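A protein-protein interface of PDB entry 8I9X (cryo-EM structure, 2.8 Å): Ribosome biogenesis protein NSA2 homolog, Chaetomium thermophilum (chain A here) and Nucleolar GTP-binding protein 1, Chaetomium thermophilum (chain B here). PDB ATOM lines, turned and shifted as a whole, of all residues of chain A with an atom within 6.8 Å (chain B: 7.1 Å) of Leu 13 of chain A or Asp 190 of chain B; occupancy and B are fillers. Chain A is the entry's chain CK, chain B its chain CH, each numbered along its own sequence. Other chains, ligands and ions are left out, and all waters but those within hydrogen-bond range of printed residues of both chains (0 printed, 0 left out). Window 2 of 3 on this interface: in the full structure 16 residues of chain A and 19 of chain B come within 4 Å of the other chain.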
ATOM      1  N   GLN A   3     -11.618  11.386   4.827  1.00  0.00           N
ATOM      2  CA  GLN A   3     -12.030  12.780   4.770  1.00  0.00           C
ATOM      3  C   GLN A   3     -13.112  13.098   3.747  1.00  0.00           C
ATOM      4  O   GLN A   3     -13.519  14.261   3.659  1.00  0.00           O
ATOM      5  CB  GLN A   3     -10.813  13.671   4.476  1.00  0.00           C
ATOM      6  CG  GLN A   3      -9.917  13.130   3.378  1.00  0.00           C
ATOM      7  CD  GLN A   3      -8.579  13.827   3.331  1.00  0.00           C
ATOM      8  OE1 GLN A   3      -8.393  14.877   3.943  1.00  0.00           O
ATOM      9  NE2 GLN A   3      -7.633  13.245   2.605  1.00  0.00           N
ATOM     10  N   ASN A   4     -13.581  12.126   2.977  1.00  0.00           N
ATOM     11  CA  ASN A   4     -14.555  12.365   1.917  1.00  0.00           C
ATOM     12  C   ASN A   4     -15.377  11.092   1.768  1.00  0.00           C
ATOM     13  O   ASN A   4     -15.507  10.301   2.706  1.00  0.00           O
ATOM     14  CB  ASN A   4     -13.861  12.822   0.627  1.00  0.00           C
ATOM     15  CG  ASN A   4     -13.569  14.308   0.630  1.00  0.00           C
ATOM     16  OD1 ASN A   4     -12.431  14.731   0.827  1.00  0.00           O
ATOM     17  ND2 ASN A   4     -14.605  15.110   0.428  1.00  0.00           N
ATOM     18  N   GLU A   8     -17.228   5.021  -0.766  1.00  0.00           N
ATOM     19  CA  GLU A   8     -17.307   5.007  -2.222  1.00  0.00           C
ATOM     20  C   GLU A   8     -15.932   4.841  -2.859  1.00  0.00           C
ATOM     21  O   GLU A   8     -15.790   4.105  -3.844  1.00  0.00           O
ATOM     22  CB  GLU A   8     -17.975   6.284  -2.729  1.00  0.00           C
ATOM     23  CG  GLU A   8     -19.490   6.263  -2.661  1.00  0.00           C
ATOM     24  CD  GLU A   8     -20.124   7.354  -3.500  1.00  0.00           C
ATOM     25  OE1 GLU A   8     -20.209   7.181  -4.734  1.00  0.00           O
ATOM     26  OE2 GLU A   8     -20.540   8.381  -2.926  1.00  0.00           O
ATOM     27  N   ARG A   9     -14.916   5.522  -2.326  1.00  0.00           N
ATOM     28  CA  ARG A   9     -13.561   5.338  -2.836  1.00  0.00           C
ATOM     29  C   ARG A   9     -13.096   3.897  -2.660  1.00  0.00           C
ATOM     30  O   ARG A   9     -12.472   3.322  -3.559  1.00  0.00           O
ATOM     31  CB  ARG A   9     -12.608   6.302  -2.130  1.00  0.00           C
ATOM     32  CG  ARG A   9     -11.190   6.297  -2.665  1.00  0.00           C
ATOM     33  CD  ARG A   9     -11.016   7.294  -3.791  1.00  0.00           C
ATOM     34  NE  ARG A   9      -9.660   7.272  -4.324  1.00  0.00           N
ATOM     35  CZ  ARG A   9      -9.363   7.186  -5.612  1.00  0.00           C
ATOM     36  NH1 ARG A   9     -10.305   7.106  -6.535  1.00  0.00           N
ATOM     37  NH2 ARG A   9      -8.085   7.182  -5.983  1.00  0.00           N
ATOM     38  N   HIS A  10     -13.387   3.304  -1.501  1.00  0.00           N
ATOM     39  CA  HIS A  10     -13.023   1.915  -1.248  1.00  0.00           C
ATOM     40  C   HIS A  10     -13.753   0.978  -2.201  1.00  0.00           C
ATOM     41  O   HIS A  10     -13.185  -0.013  -2.666  1.00  0.00           O
ATOM     42  CB  HIS A  10     -13.331   1.560   0.208  1.00  0.00           C
ATOM     43  CG  HIS A  10     -12.756   0.252   0.650  1.00  0.00           C
ATOM     44  ND1 HIS A  10     -11.456   0.120   1.086  1.00  0.00           N
ATOM     45  CD2 HIS A  10     -13.308  -0.981   0.733  1.00  0.00           C
ATOM     46  CE1 HIS A  10     -11.231  -1.139   1.415  1.00  0.00           C
ATOM     47  NE2 HIS A  10     -12.338  -1.828   1.212  1.00  0.00           N
ATOM     48  N   ARG A  11     -15.019   1.275  -2.492  1.00  0.00           N
ATOM     49  CA  ARG A  11     -15.769   0.540  -3.501  1.00  0.00           C
ATOM     50  C   ARG A  11     -15.114   0.614  -4.869  1.00  0.00           C
ATOM     51  O   ARG A  11     -14.968  -0.418  -5.533  1.00  0.00           O
ATOM     52  CB  ARG A  11     -17.189   1.101  -3.593  1.00  0.00           C
ATOM     53  CG  ARG A  11     -18.117   0.373  -4.548  1.00  0.00           C
ATOM     54  CD  ARG A  11     -19.516   0.969  -4.483  1.00  0.00           C
ATOM     55  NE  ARG A  11     -20.426   0.358  -5.444  1.00  0.00           N
ATOM     56  CZ  ARG A  11     -21.134  -0.739  -5.216  1.00  0.00           C
ATOM     57  NH1 ARG A  11     -21.086  -1.361  -4.050  1.00  0.00           N
ATOM     58  NH2 ARG A  11     -21.916  -1.219  -6.178  1.00  0.00           N
ATOM     59  N   LYS A  12     -14.721   1.808  -5.303  1.00  0.00           N
ATOM     60  CA  LYS A  12     -14.099   1.980  -6.608  1.00  0.00           C
ATOM     61  C   LYS A  12     -12.714   1.355  -6.700  1.00  0.00           C
ATOM     62  O   LYS A  12     -12.304   0.954  -7.794  1.00  0.00           O
ATOM     63  CB  LYS A  12     -14.000   3.467  -6.957  1.00  0.00           C
ATOM     64  CG  LYS A  12     -15.331   4.111  -7.293  1.00  0.00           C
ATOM     65  CD  LYS A  12     -15.150   5.555  -7.723  1.00  0.00           C
ATOM     66  CE  LYS A  12     -14.449   5.638  -9.068  1.00  0.00           C
ATOM     67  NZ  LYS A  12     -15.286   5.062 -10.158  1.00  0.00           N
ATOM     68  N   LEU A  13     -11.988   1.270  -5.590  1.00  0.00           N
ATOM     69  CA  LEU A  13     -10.621   0.760  -5.590  1.00  0.00           C
ATOM     70  C   LEU A  13     -10.516  -0.732  -5.327  1.00  0.00           C
ATOM     71  O   LEU A  13      -9.646  -1.390  -5.900  1.00  0.00           O
ATOM     72  CB  LEU A  13      -9.785   1.507  -4.547  1.00  0.00           C
ATOM     73  CG  LEU A  13      -9.233   2.870  -4.960  1.00  0.00           C
ATOM     74  CD1 LEU A  13      -8.528   3.530  -3.790  1.00  0.00           C
ATOM     75  CD2 LEU A  13      -8.293   2.729  -6.143  1.00  0.00           C
ATOM     76  N   HIS A  14     -11.373  -1.293  -4.475  1.00  0.00           N
ATOM     77  CA  HIS A  14     -11.256  -2.682  -4.065  1.00  0.00           C
ATOM     78  C   HIS A  14     -12.511  -3.514  -4.293  1.00  0.00           C
ATOM     79  O   HIS A  14     -12.410  -4.745  -4.316  1.00  0.00           O
ATOM     80  CB  HIS A  14     -10.863  -2.766  -2.582  1.00  0.00           C
ATOM     81  CG  HIS A  14      -9.702  -1.892  -2.217  1.00  0.00           C
ATOM     82  ND1 HIS A  14      -8.401  -2.207  -2.544  1.00  0.00           N
ATOM     83  CD2 HIS A  14      -9.647  -0.709  -1.560  1.00  0.00           C
ATOM     84  CE1 HIS A  14      -7.595  -1.260  -2.101  1.00  0.00           C
ATOM     85  NE2 HIS A  14      -8.325  -0.339  -1.500  1.00  0.00           N
ATOM     86  N   GLY A  15     -13.675  -2.894  -4.469  1.00  0.00           N
ATOM     87  CA  GLY A  15     -14.884  -3.641  -4.754  1.00  0.00           C
ATOM     88  C   GLY A  15     -15.719  -3.969  -3.534  1.00  0.00           C
ATOM     89  O   GLY A  15     -15.565  -3.349  -2.478  1.00  0.00           O
ATOM     90  N   VAL B 183       0.021  16.799  -3.985  1.00  0.00           N
ATOM     91  CA  VAL B 183      -0.485  16.456  -2.659  1.00  0.00           C
ATOM     92  C   VAL B 183      -0.127  15.017  -2.303  1.00  0.00           C
ATOM     93  O   VAL B 183       0.346  14.737  -1.197  1.00  0.00           O
ATOM     94  CB  VAL B 183      -2.000  16.702  -2.580  1.00  0.00           C
ATOM     95  CG1 VAL B 183      -2.600  15.943  -1.411  1.00  0.00           C
ATOM     96  CG2 VAL B 183      -2.270  18.182  -2.443  1.00  0.00           C
ATOM     97  N   ARG B 184      -0.346  14.082  -3.231  1.00  0.00           N
ATOM     98  CA  ARG B 184       0.059  12.704  -2.957  1.00  0.00           C
ATOM     99  C   ARG B 184       1.570  12.532  -2.942  1.00  0.00           C
ATOM    100  O   ARG B 184       2.066  11.608  -2.289  1.00  0.00           O
ATOM    101  CB  ARG B 184      -0.545  11.719  -3.959  1.00  0.00           C
ATOM    102  CG  ARG B 184      -1.923  12.056  -4.455  1.00  0.00           C
ATOM    103  CD  ARG B 184      -2.298  11.174  -5.627  1.00  0.00           C
ATOM    104  NE  ARG B 184      -2.195   9.756  -5.307  1.00  0.00           N
ATOM    105  CZ  ARG B 184      -3.189   9.025  -4.821  1.00  0.00           C
ATOM    106  NH1 ARG B 184      -4.380   9.549  -4.581  1.00  0.00           N
ATOM    107  NH2 ARG B 184      -2.984   7.736  -4.571  1.00  0.00           N
ATOM    108  N   THR B 187       2.348  14.029   0.719  1.00  0.00           N
ATOM    109  CA  THR B 187       1.561  13.500   1.825  1.00  0.00           C
ATOM    110  C   THR B 187       0.972  12.163   1.409  1.00  0.00           C
ATOM    111  O   THR B 187       0.955  11.814   0.227  1.00  0.00           O
ATOM    112  CB  THR B 187       0.435  14.458   2.240  1.00  0.00           C
ATOM    113  OG1 THR B 187      -0.416  14.710   1.116  1.00  0.00           O
ATOM    114  CG2 THR B 187       0.997  15.776   2.750  1.00  0.00           C
ATOM    115  N   ARG B 188       0.476  11.413   2.394  1.00  0.00           N
ATOM    116  CA  ARG B 188      -0.114  10.105   2.141  1.00  0.00           C
ATOM    117  C   ARG B 188      -1.636  10.166   2.060  1.00  0.00           C
ATOM    118  O   ARG B 188      -2.308   9.133   2.147  1.00  0.00           O
ATOM    119  CB  ARG B 188       0.338   9.099   3.203  1.00  0.00           C
ATOM    120  CG  ARG B 188      -0.367   9.192   4.544  1.00  0.00           C
ATOM    121  CD  ARG B 188       0.125   8.093   5.478  1.00  0.00           C
ATOM    122  NE  ARG B 188      -0.496   6.805   5.191  1.00  0.00           N
ATOM    123  CZ  ARG B 188      -1.628   6.375   5.732  1.00  0.00           C
ATOM    124  NH1 ARG B 188      -2.301   7.107   6.603  1.00  0.00           N
ATOM    125  NH2 ARG B 188      -2.096   5.178   5.390  1.00  0.00           N
ATOM    126  N   ALA B 189      -2.192  11.359   1.868  1.00  0.00           N
ATOM    127  CA  ALA B 189      -3.626  11.527   1.685  1.00  0.00           C
ATOM    128  C   ALA B 189      -4.016  11.075   0.285  1.00  0.00           C
ATOM    129  O   ALA B 189      -3.361  11.438  -0.697  1.00  0.00           O
ATOM    130  CB  ALA B 189      -4.032  12.984   1.905  1.00  0.00           C
ATOM    131  N   ASP B 190      -5.081  10.282   0.197  1.00  0.00           N
ATOM    132  CA  ASP B 190      -5.534   9.721  -1.074  1.00  0.00           C
ATOM    133  C   ASP B 190      -6.435  10.740  -1.761  1.00  0.00           C
ATOM    134  O   ASP B 190      -7.635  10.820  -1.500  1.00  0.00           O
ATOM    135  CB  ASP B 190      -6.257   8.399  -0.849  1.00  0.00           C
ATOM    136  CG  ASP B 190      -6.566   7.671  -2.146  1.00  0.00           C
ATOM    137  OD1 ASP B 190      -6.246   8.207  -3.228  1.00  0.00           O
ATOM    138  OD2 ASP B 190      -7.135   6.562  -2.082  1.00  0.00           O
ATOM    139  N   THR B 191      -5.844  11.531  -2.654  1.00  0.00           N
ATOM    140  CA  THR B 191      -6.591  12.489  -3.462  1.00  0.00           C
ATOM    141  C   THR B 191      -6.711  11.943  -4.877  1.00  0.00           C
ATOM    142  O   THR B 191      -5.687  11.713  -5.539  1.00  0.00           O
ATOM    143  CB  THR B 191      -5.904  13.858  -3.469  1.00  0.00           C
ATOM    144  OG1 THR B 191      -4.586  13.731  -4.016  1.00  0.00           O
ATOM    145  CG2 THR B 191      -5.806  14.405  -2.060  1.00  0.00           C
ATOM    146  N   PRO B 192      -7.926  11.684  -5.371  1.00  0.00           N
ATOM    147  CA  PRO B 192      -8.081  11.126  -6.722  1.00  0.00           C
ATOM    148  C   PRO B 192      -7.347  11.916  -7.794  1.00  0.00           C
ATOM    149  O   PRO B 192      -7.460  13.142  -7.869  1.00  0.00           O
ATOM    150  CB  PRO B 192      -9.597  11.181  -6.952  1.00  0.00           C
ATOM    151  CG  PRO B 192     -10.217  11.290  -5.590  1.00  0.00           C
ATOM    152  CD  PRO B 192      -9.148  11.535  -4.567  1.00  0.00           C
ATOM    153  N   VAL B 193      -6.591  11.212  -8.629  1.00  0.00           N
ATOM    154  CA  VAL B 193      -5.862  11.810  -9.739  1.00  0.00           C
ATOM    155  C   VAL B 193      -6.372  11.189 -11.033  1.00  0.00           C
ATOM    156  O   VAL B 193      -6.159   9.998 -11.285  1.00  0.00           O
ATOM    157  CB  VAL B 193      -4.347  11.612  -9.585  1.00  0.00           C
ATOM    158  CG1 VAL B 193      -3.633  11.925 -10.880  1.00  0.00           C
ATOM    159  CG2 VAL B 193      -3.822  12.501  -8.477  1.00  0.00           C
ATOM    160  N   PHE B 204      -9.228  18.582   0.376  1.00  0.00           N
ATOM    161  CA  PHE B 204      -8.536  17.426   0.937  1.00  0.00           C
ATOM    162  C   PHE B 204      -7.395  17.877   1.835  1.00  0.00           C
ATOM    163  O   PHE B 204      -6.782  18.919   1.591  1.00  0.00           O
ATOM    164  CB  PHE B 204      -8.010  16.501  -0.160  1.00  0.00           C
ATOM    165  CG  PHE B 204      -9.058  15.598  -0.739  1.00  0.00           C
ATOM    166  CD1 PHE B 204     -10.079  16.105  -1.519  1.00  0.00           C
ATOM    167  CD2 PHE B 204      -9.025  14.238  -0.491  1.00  0.00           C
ATOM    168  CE1 PHE B 204     -11.041  15.271  -2.048  1.00  0.00           C
ATOM    169  CE2 PHE B 204      -9.984  13.400  -1.016  1.00  0.00           C
ATOM    170  CZ  PHE B 204     -10.992  13.918  -1.797  1.00  0.00           C
ATOM    171  N   VAL B 205      -7.112  17.089   2.870  1.00  0.00           N
ATOM    172  CA  VAL B 205      -6.116  17.426   3.879  1.00  0.00           C
ATOM    173  C   VAL B 205      -5.077  16.317   3.944  1.00  0.00           C
ATOM    174  O   VAL B 205      -5.425  15.133   4.040  1.00  0.00           O
ATOM    175  CB  VAL B 205      -6.764  17.645   5.256  1.00  0.00           C
ATOM    176  CG1 VAL B 205      -5.725  18.087   6.270  1.00  0.00           C
ATOM    177  CG2 VAL B 205      -7.877  18.661   5.155  1.00  0.00           C
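Of the 10 printed residues of chain A, 4 touch a printed residue of chain B. Printed residues of chain B that touch a printed residue of chain A: Ala 189, Asp 190, Phe 204 and Val 205. Hydrophobic or aromatic side chains of chain B that line the printed part of chain A: Ala 189, Phe 204 and Val 205. Among the printed residues, 6 pairs touch across the chains. Among the printed residues, Asp or Glu carboxylates within 4 Å of a Lys or Arg side-chain nitrogen of the other chain: Arg 9 of chain A with Asp 190 of chain B.
Ala 189 of chain B touches Gln 3 of chain A (CB to NE2, 3.7 Å). Gln 3 of chain A touches Phe 204 of chain B. OD1 of Asn 4 of chain A touches CZ of Phe 204 of chain B, at 3.1 Å. Leu 13 of chain A touches Asp 190 of chain B.
The guanidinium group of Arg 184 of chain B lies within salt-bridge range of the side-chain carboxylate of Asp 190 of chain B (2.7 Å).
Of chain B, only Asp 190 (3.7 Å) comes within 4 Å of Leu 13 of chain A. Asp 190 of chain B touches just these residues of chain A: Arg 9 and Leu 13. Of the printed residues of chain B, Arg 9 of chain A touches Asp 190. Of the printed residues of chain A, Ala 189 of chain B touches Gln 3. Arg 11 of chain A touches none of the printed residues of chain B. The nearest residue of chain B that does not touch Leu 13 of chain A is Arg 184 of chain B (7.0 Å). The nearest residue of chain A that does not touch Asp 190 of chain B is Gln 3 of chain A (4.6 Å).
NE of Arg 9 of chain A lies within salt-bridge range of OD2 of Asp 190 of chain B. The backbone NH (N) of Val 205 of chain B is in hydrogen-bond range of the side-chain amide oxygen (OE1) of Gln 3 of chain A, 2.8 Å away.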
